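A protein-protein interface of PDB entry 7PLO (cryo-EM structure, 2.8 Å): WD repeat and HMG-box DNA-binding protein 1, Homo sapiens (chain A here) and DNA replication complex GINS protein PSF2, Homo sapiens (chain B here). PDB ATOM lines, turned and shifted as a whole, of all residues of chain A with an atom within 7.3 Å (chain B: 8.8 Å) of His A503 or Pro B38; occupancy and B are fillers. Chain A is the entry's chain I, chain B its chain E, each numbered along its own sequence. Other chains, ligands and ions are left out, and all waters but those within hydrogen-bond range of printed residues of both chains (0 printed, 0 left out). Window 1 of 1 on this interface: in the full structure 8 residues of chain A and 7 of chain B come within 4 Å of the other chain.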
ATOM      1  N   TRP A 481     -16.150 -13.361   9.291  1.00  0.00           N
ATOM      2  CA  TRP A 481     -17.069 -12.259   9.555  1.00  0.00           C
ATOM      3  C   TRP A 481     -17.943 -12.697  10.719  1.00  0.00           C
ATOM      4  O   TRP A 481     -18.714 -13.654  10.590  1.00  0.00           O
ATOM      5  CB  TRP A 481     -17.910 -11.918   8.308  1.00  0.00           C
ATOM      6  CG  TRP A 481     -18.826 -10.674   8.373  1.00  0.00           C
ATOM      7  CD1 TRP A 481     -19.381 -10.089   9.484  1.00  0.00           C
ATOM      8  CD2 TRP A 481     -19.283  -9.894   7.256  1.00  0.00           C
ATOM      9  NE1 TRP A 481     -20.145  -9.008   9.127  1.00  0.00           N
ATOM     10  CE2 TRP A 481     -20.100  -8.865   7.767  1.00  0.00           C
ATOM     11  CE3 TRP A 481     -19.076  -9.965   5.875  1.00  0.00           C
ATOM     12  CZ2 TRP A 481     -20.708  -7.917   6.946  1.00  0.00           C
ATOM     13  CZ3 TRP A 481     -19.681  -9.023   5.062  1.00  0.00           C
ATOM     14  CH2 TRP A 481     -20.487  -8.014   5.601  1.00  0.00           C
ATOM     15  N   ASN A 482     -17.819 -11.999  11.845  1.00  0.00           N
ATOM     16  CA  ASN A 482     -18.600 -12.276  13.045  1.00  0.00           C
ATOM     17  C   ASN A 482     -19.056 -10.936  13.620  1.00  0.00           C
ATOM     18  O   ASN A 482     -18.925  -9.889  12.979  1.00  0.00           O
ATOM     19  CB  ASN A 482     -17.782 -13.126  14.030  1.00  0.00           C
ATOM     20  CG  ASN A 482     -16.416 -12.530  14.344  1.00  0.00           C
ATOM     21  OD1 ASN A 482     -16.209 -11.321  14.259  1.00  0.00           O
ATOM     22  ND2 ASN A 482     -15.475 -13.389  14.715  1.00  0.00           N
ATOM     23  N   SER A 483     -19.592 -10.962  14.839  1.00  0.00           N
ATOM     24  CA  SER A 483     -20.057  -9.750  15.500  1.00  0.00           C
ATOM     25  C   SER A 483     -18.924  -8.893  16.059  1.00  0.00           C
ATOM     26  O   SER A 483     -19.208  -7.835  16.631  1.00  0.00           O
ATOM     27  CB  SER A 483     -21.032 -10.114  16.622  1.00  0.00           C
ATOM     28  OG  SER A 483     -22.206 -10.704  16.092  1.00  0.00           O
ATOM     29  N   ILE A 484     -17.668  -9.321  15.924  1.00  0.00           N
ATOM     30  CA  ILE A 484     -16.521  -8.492  16.288  1.00  0.00           C
ATOM     31  C   ILE A 484     -16.051  -7.664  15.102  1.00  0.00           C
ATOM     32  O   ILE A 484     -15.759  -6.474  15.244  1.00  0.00           O
ATOM     33  CB  ILE A 484     -15.372  -9.372  16.838  1.00  0.00           C
ATOM     34  CG1 ILE A 484     -15.860 -10.328  17.939  1.00  0.00           C
ATOM     35  CG2 ILE A 484     -14.222  -8.499  17.358  1.00  0.00           C
ATOM     36  CD1 ILE A 484     -16.532  -9.663  19.133  1.00  0.00           C
ATOM     37  N   GLY A 485     -15.966  -8.274  13.929  1.00  0.00           N
ATOM     38  CA  GLY A 485     -15.420  -7.582  12.782  1.00  0.00           C
ATOM     39  C   GLY A 485     -15.338  -8.488  11.579  1.00  0.00           C
ATOM     40  O   GLY A 485     -16.038  -9.498  11.491  1.00  0.00           O
ATOM     41  N   ILE A 486     -14.471  -8.100  10.646  1.00  0.00           N
ATOM     42  CA  ILE A 486     -14.248  -8.828   9.403  1.00  0.00           C
ATOM     43  C   ILE A 486     -12.746  -8.921   9.175  1.00  0.00           C
ATOM     44  O   ILE A 486     -11.993  -8.004   9.528  1.00  0.00           O
ATOM     45  CB  ILE A 486     -14.952  -8.147   8.203  1.00  0.00           C
ATOM     46  CG1 ILE A 486     -16.459  -8.023   8.469  1.00  0.00           C
ATOM     47  CG2 ILE A 486     -14.698  -8.914   6.887  1.00  0.00           C
ATOM     48  CD1 ILE A 486     -16.882  -6.672   9.000  1.00  0.00           C
ATOM     49  N   GLU A 501     -10.428  -5.603  10.146  1.00  0.00           N
ATOM     50  CA  GLU A 501     -11.244  -4.457  10.520  1.00  0.00           C
ATOM     51  C   GLU A 501     -12.298  -4.906  11.522  1.00  0.00           C
ATOM     52  O   GLU A 501     -12.619  -6.092  11.625  1.00  0.00           O
ATOM     53  CB  GLU A 501     -11.915  -3.807   9.302  1.00  0.00           C
ATOM     54  CG  GLU A 501     -12.773  -4.746   8.464  1.00  0.00           C
ATOM     55  CD  GLU A 501     -13.403  -4.046   7.279  1.00  0.00           C
ATOM     56  OE1 GLU A 501     -14.114  -3.041   7.490  1.00  0.00           O
ATOM     57  OE2 GLU A 501     -13.181  -4.496   6.135  1.00  0.00           O
ATOM     58  N   PHE A 502     -12.850  -3.928  12.235  1.00  0.00           N
ATOM     59  CA  PHE A 502     -13.768  -4.155  13.340  1.00  0.00           C
ATOM     60  C   PHE A 502     -15.066  -3.400  13.093  1.00  0.00           C
ATOM     61  O   PHE A 502     -15.069  -2.326  12.485  1.00  0.00           O
ATOM     62  CB  PHE A 502     -13.141  -3.712  14.672  1.00  0.00           C
ATOM     63  CG  PHE A 502     -11.909  -4.489  15.052  1.00  0.00           C
ATOM     64  CD1 PHE A 502     -10.675  -4.180  14.499  1.00  0.00           C
ATOM     65  CD2 PHE A 502     -11.983  -5.526  15.965  1.00  0.00           C
ATOM     66  CE1 PHE A 502      -9.547  -4.895  14.843  1.00  0.00           C
ATOM     67  CE2 PHE A 502     -10.855  -6.241  16.315  1.00  0.00           C
ATOM     68  CZ  PHE A 502      -9.636  -5.924  15.753  1.00  0.00           C
ATOM     69  N   HIS A 503     -16.174  -3.985  13.557  1.00  0.00           N
ATOM     70  CA  HIS A 503     -17.461  -3.305  13.460  1.00  0.00           C
ATOM     71  C   HIS A 503     -17.438  -1.992  14.229  1.00  0.00           C
ATOM     72  O   HIS A 503     -17.904  -0.965  13.726  1.00  0.00           O
ATOM     73  CB  HIS A 503     -18.583  -4.202  13.988  1.00  0.00           C
ATOM     74  CG  HIS A 503     -18.970  -5.317  13.064  1.00  0.00           C
ATOM     75  ND1 HIS A 503     -19.961  -6.222  13.376  1.00  0.00           N
ATOM     76  CD2 HIS A 503     -18.509  -5.672  11.841  1.00  0.00           C
ATOM     77  CE1 HIS A 503     -20.092  -7.087  12.386  1.00  0.00           C
ATOM     78  NE2 HIS A 503     -19.223  -6.776  11.443  1.00  0.00           N
ATOM     79  N   ASP A 504     -16.890  -2.009  15.441  1.00  0.00           N
ATOM     80  CA  ASP A 504     -16.736  -0.826  16.279  1.00  0.00           C
ATOM     81  C   ASP A 504     -15.257  -0.463  16.309  1.00  0.00           C
ATOM     82  O   ASP A 504     -14.431  -1.251  16.781  1.00  0.00           O
ATOM     83  CB  ASP A 504     -17.263  -1.091  17.689  1.00  0.00           C
ATOM     84  CG  ASP A 504     -17.571   0.185  18.449  1.00  0.00           C
ATOM     85  OD1 ASP A 504     -16.917   1.214  18.182  1.00  0.00           O
ATOM     86  OD2 ASP A 504     -18.469   0.157  19.316  1.00  0.00           O
ATOM     87  N   THR A 505     -14.928   0.726  15.808  1.00  0.00           N
ATOM     88  CA  THR A 505     -13.536   1.147  15.697  1.00  0.00           C
ATOM     89  C   THR A 505     -12.943   1.613  17.022  1.00  0.00           C
ATOM     90  O   THR A 505     -11.744   1.908  17.070  1.00  0.00           O
ATOM     91  CB  THR A 505     -13.402   2.257  14.651  1.00  0.00           C
ATOM     92  OG1 THR A 505     -14.333   3.308  14.935  1.00  0.00           O
ATOM     93  CG2 THR A 505     -13.664   1.704  13.255  1.00  0.00           C
ATOM     94  N   SER A 506     -13.741   1.695  18.090  1.00  0.00           N
ATOM     95  CA  SER A 506     -13.178   1.893  19.420  1.00  0.00           C
ATOM     96  C   SER A 506     -12.414   0.668  19.912  1.00  0.00           C
ATOM     97  O   SER A 506     -11.622   0.787  20.853  1.00  0.00           O
ATOM     98  CB  SER A 506     -14.286   2.236  20.416  1.00  0.00           C
ATOM     99  OG  SER A 506     -15.134   1.123  20.637  1.00  0.00           O
ATOM    100  N   ILE A 507     -12.632  -0.499  19.302  1.00  0.00           N
ATOM    101  CA  ILE A 507     -11.978  -1.722  19.760  1.00  0.00           C
ATOM    102  C   ILE A 507     -10.487  -1.672  19.443  1.00  0.00           C
ATOM    103  O   ILE A 507      -9.639  -1.741  20.340  1.00  0.00           O
ATOM    104  CB  ILE A 507     -12.653  -2.957  19.130  1.00  0.00           C
ATOM    105  CG1 ILE A 507     -14.086  -3.121  19.665  1.00  0.00           C
ATOM    106  CG2 ILE A 507     -11.836  -4.229  19.405  1.00  0.00           C
ATOM    107  CD1 ILE A 507     -14.990  -3.991  18.798  1.00  0.00           C
ATOM    108  N   LEU A 524     -11.307 -14.320  14.725  1.00  0.00           N
ATOM    109  CA  LEU A 524     -11.281 -12.991  15.324  1.00  0.00           C
ATOM    110  C   LEU A 524     -12.048 -13.015  16.641  1.00  0.00           C
ATOM    111  O   LEU A 524     -13.031 -13.744  16.786  1.00  0.00           O
ATOM    112  CB  LEU A 524     -11.894 -11.963  14.353  1.00  0.00           C
ATOM    113  CG  LEU A 524     -12.084 -10.503  14.774  1.00  0.00           C
ATOM    114  CD1 LEU A 524     -10.761  -9.851  15.094  1.00  0.00           C
ATOM    115  CD2 LEU A 524     -12.798  -9.742  13.669  1.00  0.00           C
ATOM    116  N   VAL A 710     -23.981 -14.701  10.109  1.00  0.00           N
ATOM    117  CA  VAL A 710     -22.887 -13.988  10.752  1.00  0.00           C
ATOM    118  C   VAL A 710     -22.857 -14.238  12.256  1.00  0.00           C
ATOM    119  O   VAL A 710     -21.779 -14.358  12.842  1.00  0.00           O
ATOM    120  CB  VAL A 710     -22.988 -12.474  10.438  1.00  0.00           C
ATOM    121  CG1 VAL A 710     -22.159 -11.609  11.414  1.00  0.00           C
ATOM    122  CG2 VAL A 710     -22.569 -12.203   8.985  1.00  0.00           C
ATOM    123  N   ARG A 720     -28.132 -12.462  12.800  1.00  0.00           N
ATOM    124  CA  ARG A 720     -27.456 -11.627  11.817  1.00  0.00           C
ATOM    125  C   ARG A 720     -27.168 -12.476  10.589  1.00  0.00           C
ATOM    126  O   ARG A 720     -26.515 -13.518  10.696  1.00  0.00           O
ATOM    127  CB  ARG A 720     -26.160 -11.050  12.388  1.00  0.00           C
ATOM    128  CG  ARG A 720     -26.334  -9.820  13.279  1.00  0.00           C
ATOM    129  CD  ARG A 720     -26.759 -10.185  14.694  1.00  0.00           C
ATOM    130  NE  ARG A 720     -26.976  -9.015  15.539  1.00  0.00           N
ATOM    131  CZ  ARG A 720     -26.018  -8.271  16.079  1.00  0.00           C
ATOM    132  NH1 ARG A 720     -24.736  -8.490  15.828  1.00  0.00           N
ATOM    133  NH2 ARG A 720     -26.356  -7.280  16.899  1.00  0.00           N
ATOM    134  N   ARG A 735     -19.669  -4.002  -0.175  1.00  0.00           N
ATOM    135  CA  ARG A 735     -19.801  -4.533   1.180  1.00  0.00           C
ATOM    136  C   ARG A 735     -21.261  -4.898   1.449  1.00  0.00           C
ATOM    137  O   ARG A 735     -22.126  -4.019   1.344  1.00  0.00           O
ATOM    138  CB  ARG A 735     -19.304  -3.501   2.195  1.00  0.00           C
ATOM    139  CG  ARG A 735     -19.342  -3.935   3.673  1.00  0.00           C
ATOM    140  CD  ARG A 735     -18.450  -5.141   3.974  1.00  0.00           C
ATOM    141  NE  ARG A 735     -17.036  -4.874   3.722  1.00  0.00           N
ATOM    142  CZ  ARG A 735     -16.177  -4.348   4.590  1.00  0.00           C
ATOM    143  NH1 ARG A 735     -16.544  -3.991   5.813  1.00  0.00           N
ATOM    144  NH2 ARG A 735     -14.911  -4.173   4.220  1.00  0.00           N
ATOM    145  N   VAL A 738     -26.008  -6.293   6.582  1.00  0.00           N
ATOM    146  CA  VAL A 738     -26.505  -7.376   7.425  1.00  0.00           C
ATOM    147  C   VAL A 738     -27.983  -7.150   7.710  1.00  0.00           C
ATOM    148  O   VAL A 738     -28.377  -6.091   8.211  1.00  0.00           O
ATOM    149  CB  VAL A 738     -25.691  -7.463   8.730  1.00  0.00           C
ATOM    150  CG1 VAL A 738     -26.390  -8.373   9.761  1.00  0.00           C
ATOM    151  CG2 VAL A 738     -24.259  -7.938   8.438  1.00  0.00           C
ATOM    152  N   ILE B  17     -27.848   3.957   7.062  1.00  0.00           N
ATOM    153  CA  ILE B  17     -26.414   3.974   7.316  1.00  0.00           C
ATOM    154  C   ILE B  17     -26.048   2.729   8.114  1.00  0.00           C
ATOM    155  O   ILE B  17     -26.896   2.099   8.747  1.00  0.00           O
ATOM    156  CB  ILE B  17     -25.960   5.255   8.060  1.00  0.00           C
ATOM    157  CG1 ILE B  17     -26.656   5.423   9.426  1.00  0.00           C
ATOM    158  CG2 ILE B  17     -26.238   6.471   7.198  1.00  0.00           C
ATOM    159  CD1 ILE B  17     -26.021   6.480  10.297  1.00  0.00           C
ATOM    160  N   ILE B  18     -24.764   2.399   8.091  1.00  0.00           N
ATOM    161  CA  ILE B  18     -24.186   1.339   8.908  1.00  0.00           C
ATOM    162  C   ILE B  18     -23.198   1.985   9.878  1.00  0.00           C
ATOM    163  O   ILE B  18     -22.079   2.328   9.497  1.00  0.00           O
ATOM    164  CB  ILE B  18     -23.501   0.271   8.035  1.00  0.00           C
ATOM    165  CG1 ILE B  18     -24.565  -0.565   7.319  1.00  0.00           C
ATOM    166  CG2 ILE B  18     -22.597  -0.634   8.881  1.00  0.00           C
ATOM    167  CD1 ILE B  18     -24.067  -1.312   6.102  1.00  0.00           C
ATOM    168  N   PRO B  19     -23.576   2.183  11.148  1.00  0.00           N
ATOM    169  CA  PRO B  19     -22.645   2.824  12.081  1.00  0.00           C
ATOM    170  C   PRO B  19     -21.430   1.962  12.378  1.00  0.00           C
ATOM    171  O   PRO B  19     -21.466   0.734  12.269  1.00  0.00           O
ATOM    172  CB  PRO B  19     -23.486   3.023  13.348  1.00  0.00           C
ATOM    173  CG  PRO B  19     -24.874   2.917  12.919  1.00  0.00           C
ATOM    174  CD  PRO B  19     -24.871   1.939  11.810  1.00  0.00           C
ATOM    175  N   ASN B  20     -20.335   2.638  12.739  1.00  0.00           N
ATOM    176  CA  ASN B  20     -19.186   2.012  13.384  1.00  0.00           C
ATOM    177  C   ASN B  20     -19.058   2.432  14.847  1.00  0.00           C
ATOM    178  O   ASN B  20     -17.967   2.352  15.419  1.00  0.00           O
ATOM    179  CB  ASN B  20     -17.897   2.317  12.612  1.00  0.00           C
ATOM    180  CG  ASN B  20     -17.639   3.807  12.426  1.00  0.00           C
ATOM    181  OD1 ASN B  20     -17.999   4.634  13.261  1.00  0.00           O
ATOM    182  ND2 ASN B  20     -17.000   4.149  11.317  1.00  0.00           N
ATOM    183  N   PHE B  21     -20.155   2.884  15.456  1.00  0.00           N
ATOM    184  CA  PHE B  21     -20.177   3.342  16.836  1.00  0.00           C
ATOM    185  C   PHE B  21     -21.441   2.814  17.495  1.00  0.00           C
ATOM    186  O   PHE B  21     -22.415   2.468  16.821  1.00  0.00           O
ATOM    187  CB  PHE B  21     -20.129   4.875  16.931  1.00  0.00           C
ATOM    188  CG  PHE B  21     -21.313   5.565  16.308  1.00  0.00           C
ATOM    189  CD1 PHE B  21     -21.329   5.852  14.957  1.00  0.00           C
ATOM    190  CD2 PHE B  21     -22.402   5.942  17.077  1.00  0.00           C
ATOM    191  CE1 PHE B  21     -22.407   6.493  14.383  1.00  0.00           C
ATOM    192  CE2 PHE B  21     -23.484   6.574  16.504  1.00  0.00           C
ATOM    193  CZ  PHE B  21     -23.486   6.849  15.157  1.00  0.00           C
ATOM    194  N   SER B  22     -21.413   2.762  18.824  1.00  0.00           N
ATOM    195  CA  SER B  22     -22.530   2.292  19.631  1.00  0.00           C
ATOM    196  C   SER B  22     -23.166   3.473  20.346  1.00  0.00           C
ATOM    197  O   SER B  22     -22.475   4.244  21.020  1.00  0.00           O
ATOM    198  CB  SER B  22     -22.070   1.245  20.645  1.00  0.00           C
ATOM    199  OG  SER B  22     -23.170   0.753  21.391  1.00  0.00           O
ATOM    200  N   LEU B  23     -24.481   3.611  20.196  1.00  0.00           N
ATOM    201  CA  LEU B  23     -25.223   4.702  20.809  1.00  0.00           C
ATOM    202  C   LEU B  23     -26.670   4.279  20.989  1.00  0.00           C
ATOM    203  O   LEU B  23     -27.267   3.694  20.080  1.00  0.00           O
ATOM    204  CB  LEU B  23     -25.143   5.967  19.956  1.00  0.00           C
ATOM    205  CG  LEU B  23     -25.611   7.273  20.591  1.00  0.00           C
ATOM    206  CD1 LEU B  23     -24.609   7.773  21.585  1.00  0.00           C
ATOM    207  CD2 LEU B  23     -25.849   8.304  19.532  1.00  0.00           C
ATOM    208  N   PRO B  35     -31.836   2.502  18.223  1.00  0.00           N
ATOM    209  CA  PRO B  35     -30.428   2.557  18.655  1.00  0.00           C
ATOM    210  C   PRO B  35     -29.429   2.300  17.535  1.00  0.00           C
ATOM    211  O   PRO B  35     -29.723   1.644  16.542  1.00  0.00           O
ATOM    212  CB  PRO B  35     -30.356   1.460  19.727  1.00  0.00           C
ATOM    213  CG  PRO B  35     -31.420   0.493  19.346  1.00  0.00           C
ATOM    214  CD  PRO B  35     -32.532   1.341  18.800  1.00  0.00           C
ATOM    215  N   PHE B  36     -28.226   2.841  17.710  1.00  0.00           N
ATOM    216  CA  PHE B  36     -27.131   2.691  16.759  1.00  0.00           C
ATOM    217  C   PHE B  36     -26.234   1.558  17.240  1.00  0.00           C
ATOM    218  O   PHE B  36     -25.587   1.674  18.285  1.00  0.00           O
ATOM    219  CB  PHE B  36     -26.335   3.987  16.631  1.00  0.00           C
ATOM    220  CG  PHE B  36     -27.131   5.157  16.132  1.00  0.00           C
ATOM    221  CD1 PHE B  36     -27.940   5.883  16.983  1.00  0.00           C
ATOM    222  CD2 PHE B  36     -27.041   5.555  14.816  1.00  0.00           C
ATOM    223  CE1 PHE B  36     -28.655   6.953  16.525  1.00  0.00           C
ATOM    224  CE2 PHE B  36     -27.753   6.630  14.361  1.00  0.00           C
ATOM    225  CZ  PHE B  36     -28.559   7.328  15.216  1.00  0.00           C
ATOM    226  N   ASN B  37     -26.201   0.465  16.477  1.00  0.00           N
ATOM    227  CA  ASN B  37     -25.398  -0.711  16.771  1.00  0.00           C
ATOM    228  C   ASN B  37     -24.296  -0.840  15.726  1.00  0.00           C
ATOM    229  O   ASN B  37     -24.601  -0.691  14.535  1.00  0.00           O
ATOM    230  CB  ASN B  37     -26.280  -1.961  16.764  1.00  0.00           C
ATOM    231  CG  ASN B  37     -27.265  -1.978  17.917  1.00  0.00           C
ATOM    232  OD1 ASN B  37     -26.876  -1.858  19.079  1.00  0.00           O
ATOM    233  ND2 ASN B  37     -28.549  -2.109  17.604  1.00  0.00           N
ATOM    234  N   PRO B  38     -23.027  -1.079  16.086  1.00  0.00           N
ATOM    235  CA  PRO B  38     -21.988  -1.175  15.048  1.00  0.00           C
ATOM    236  C   PRO B  38     -22.237  -2.325  14.081  1.00  0.00           C
ATOM    237  O   PRO B  38     -22.540  -3.449  14.486  1.00  0.00           O
ATOM    238  CB  PRO B  38     -20.699  -1.393  15.851  1.00  0.00           C
ATOM    239  CG  PRO B  38     -20.977  -0.863  17.178  1.00  0.00           C
ATOM    240  CD  PRO B  38     -22.422  -1.120  17.433  1.00  0.00           C
ATOM    241  N   GLY B  39     -22.101  -2.028  12.790  1.00  0.00           N
ATOM    242  CA  GLY B  39     -22.156  -3.028  11.751  1.00  0.00           C
ATOM    243  C   GLY B  39     -23.535  -3.357  11.219  1.00  0.00           C
ATOM    244  O   GLY B  39     -23.630  -4.127  10.254  1.00  0.00           O
ATOM    245  N   LEU B  40     -24.617  -2.791  11.808  1.00  0.00           N
ATOM    246  CA  LEU B  40     -25.993  -3.078  11.416  1.00  0.00           C
ATOM    247  C   LEU B  40     -26.633  -1.864  10.741  1.00  0.00           C
ATOM    248  O   LEU B  40     -26.252  -0.727  11.031  1.00  0.00           O
ATOM    249  CB  LEU B  40     -26.851  -3.469  12.625  1.00  0.00           C
ATOM    250  CG  LEU B  40     -26.472  -4.698  13.454  1.00  0.00           C
ATOM    251  CD1 LEU B  40     -27.560  -4.947  14.483  1.00  0.00           C
ATOM    252  CD2 LEU B  40     -26.251  -5.941  12.601  1.00  0.00           C
ATOM    253  N   PRO B  41     -27.612  -2.049   9.847  1.00  0.00           N
ATOM    254  CA  PRO B  41     -28.262  -0.882   9.240  1.00  0.00           C
ATOM    255  C   PRO B  41     -29.208  -0.182  10.205  1.00  0.00           C
ATOM    256  O   PRO B  41     -29.872  -0.817  11.028  1.00  0.00           O
ATOM    257  CB  PRO B  41     -29.019  -1.477   8.049  1.00  0.00           C
ATOM    258  CG  PRO B  41     -29.288  -2.865   8.438  1.00  0.00           C
ATOM    259  CD  PRO B  41     -28.102  -3.301   9.238  1.00  0.00           C
ATOM    260  N   VAL B  42     -29.259   1.143  10.092  1.00  0.00           N
ATOM    261  CA  VAL B  42     -30.218   1.970  10.819  1.00  0.00           C
ATOM    262  C   VAL B  42     -30.592   3.146   9.928  1.00  0.00           C
ATOM    263  O   VAL B  42     -29.745   3.690   9.213  1.00  0.00           O
ATOM    264  CB  VAL B  42     -29.657   2.435  12.186  1.00  0.00           C
ATOM    265  CG1 VAL B  42     -28.437   3.343  12.019  1.00  0.00           C
ATOM    266  CG2 VAL B  42     -30.735   3.127  13.019  1.00  0.00           C
ATOM    267  N   GLN B  56     -16.737  10.341   9.567  1.00  0.00           N
ATOM    268  CA  GLN B  56     -16.188   8.994   9.410  1.00  0.00           C
ATOM    269  C   GLN B  56     -16.831   7.986  10.354  1.00  0.00           C
ATOM    270  O   GLN B  56     -16.219   6.965  10.677  1.00  0.00           O
ATOM    271  CB  GLN B  56     -14.671   8.972   9.609  1.00  0.00           C
ATOM    272  CG  GLN B  56     -13.904   9.979   8.789  1.00  0.00           C
ATOM    273  CD  GLN B  56     -12.413   9.725   8.836  1.00  0.00           C
ATOM    274  OE1 GLN B  56     -11.959   8.605   8.613  1.00  0.00           O
ATOM    275  NE2 GLN B  56     -11.644  10.763   9.136  1.00  0.00           N
ATOM    276  N   LYS B  57     -18.062   8.247  10.790  1.00  0.00           N
ATOM    277  CA  LYS B  57     -18.720   7.442  11.808  1.00  0.00           C
ATOM    278  C   LYS B  57     -19.724   6.442  11.241  1.00  0.00           C
ATOM    279  O   LYS B  57     -20.419   5.784  12.020  1.00  0.00           O
ATOM    280  CB  LYS B  57     -19.414   8.354  12.818  1.00  0.00           C
ATOM    281  CG  LYS B  57     -18.466   9.306  13.527  1.00  0.00           C
ATOM    282  CD  LYS B  57     -18.920   9.604  14.944  1.00  0.00           C
ATOM    283  CE  LYS B  57     -18.516   8.502  15.915  1.00  0.00           C
ATOM    284  NZ  LYS B  57     -17.093   8.607  16.333  1.00  0.00           N
ATOM    285  N   CYS B  58     -19.827   6.305   9.921  1.00  0.00           N
ATOM    286  CA  CYS B  58     -20.780   5.356   9.356  1.00  0.00           C
ATOM    287  C   CYS B  58     -20.466   5.108   7.888  1.00  0.00           C
ATOM    288  O   CYS B  58     -19.687   5.828   7.260  1.00  0.00           O
ATOM    289  CB  CYS B  58     -22.220   5.853   9.505  1.00  0.00           C
ATOM    290  SG  CYS B  58     -22.593   7.320   8.531  1.00  0.00           S
ATOM    291  N   ARG B  59     -21.092   4.058   7.361  1.00  0.00           N
ATOM    292  CA  ARG B  59     -21.109   3.731   5.942  1.00  0.00           C
ATOM    293  C   ARG B  59     -22.528   3.936   5.431  1.00  0.00           C
ATOM    294  O   ARG B  59     -23.475   3.362   5.979  1.00  0.00           O
ATOM    295  CB  ARG B  59     -20.645   2.283   5.721  1.00  0.00           C
ATOM    296  CG  ARG B  59     -20.890   1.676   4.328  1.00  0.00           C
ATOM    297  CD  ARG B  59     -20.424   0.226   4.269  1.00  0.00           C
ATOM    298  NE  ARG B  59     -18.970   0.100   4.209  1.00  0.00           N
ATOM    299  CZ  ARG B  59     -18.237   0.116   3.100  1.00  0.00           C
ATOM    300  NH1 ARG B  59     -18.779   0.290   1.902  1.00  0.00           N
ATOM    301  NH2 ARG B  59     -16.920  -0.047   3.194  1.00  0.00           N
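Printed residues of chain A that touch a printed residue of chain B: His A503, Asp A504, Thr A505, Arg A720, Arg A735 and Val A738.
Hydrophobic or aromatic side chains of chain A within 4 Å of the printed part of chain B: His A503 and Val A738.
Among the printed residues, no Asp or Glu carboxylate lies within 4 Å of a Lys or Arg side-chain nitrogen of the other chain.
Among the printed residues, merely in contact across the chains: His A503 with Asn B20 (3.3 Å), His A503 with Pro B38 (3.5 Å), Asp A504 with Ser B22 (3.96 Å), Asp A504 with Pro B38 (3.4 Å), Arg A720 with Leu B40 (3.6 Å), Arg A735 with Arg B59 (3.8 Å), Val A738 with Leu B40 (3.7 Å) and Val A738 with Pro B41 (3.0 Å).
The backbone carbonyl oxygen (O) of Asn B20 lies within hydrogen-bond range of the backbone NH (N) of Thr A505, at 3.5 Å.
OD1 of Asp A504 lies close to O of Asn B20 (3.2 Å).
ND2 of Asn B20 sits at hydrogen-bond distance from O of Gln B56 (3.0 Å).
OD1 of Asn B20 lies close to O of Lys B57 (3.0 Å).
The indole nitrogen of Trp A481 sits at hydrogen-bond distance from a ring nitrogen (NE2) of His A503 (3.3 Å).
The backbone carbonyl oxygen of Asn A482 lies close to a ring nitrogen (NE2) of His A503 (3.5 Å).
The side-chain hydroxyl (OG) of Ser A483 sits at hydrogen-bond distance from the guanidinium group (NH1) of Arg A720 (3.4 Å).
N of His A503 lies within hydrogen-bond range of O of Ile A484, 3.0 Å away.
Of chain B, only Asn B20 (3.3 Å) and Pro B38 (3.5 Å) come within 4 Å of His A503.
Of the printed residues of chain B, Thr A505 touches Asn B20.
Printed residues of chain B within 4 Å of Arg A735: Arg B59.
Of the printed residues of chain B, Val A738 touches Leu B40 and Pro B41.
Pro B38 touches two residues of chain A.
Of the printed residues of chain A, Pro B41 touches Val A738.
The nearest printed residue of chain B that does not touch Val A738 is Gly B39 (4.2 Å).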
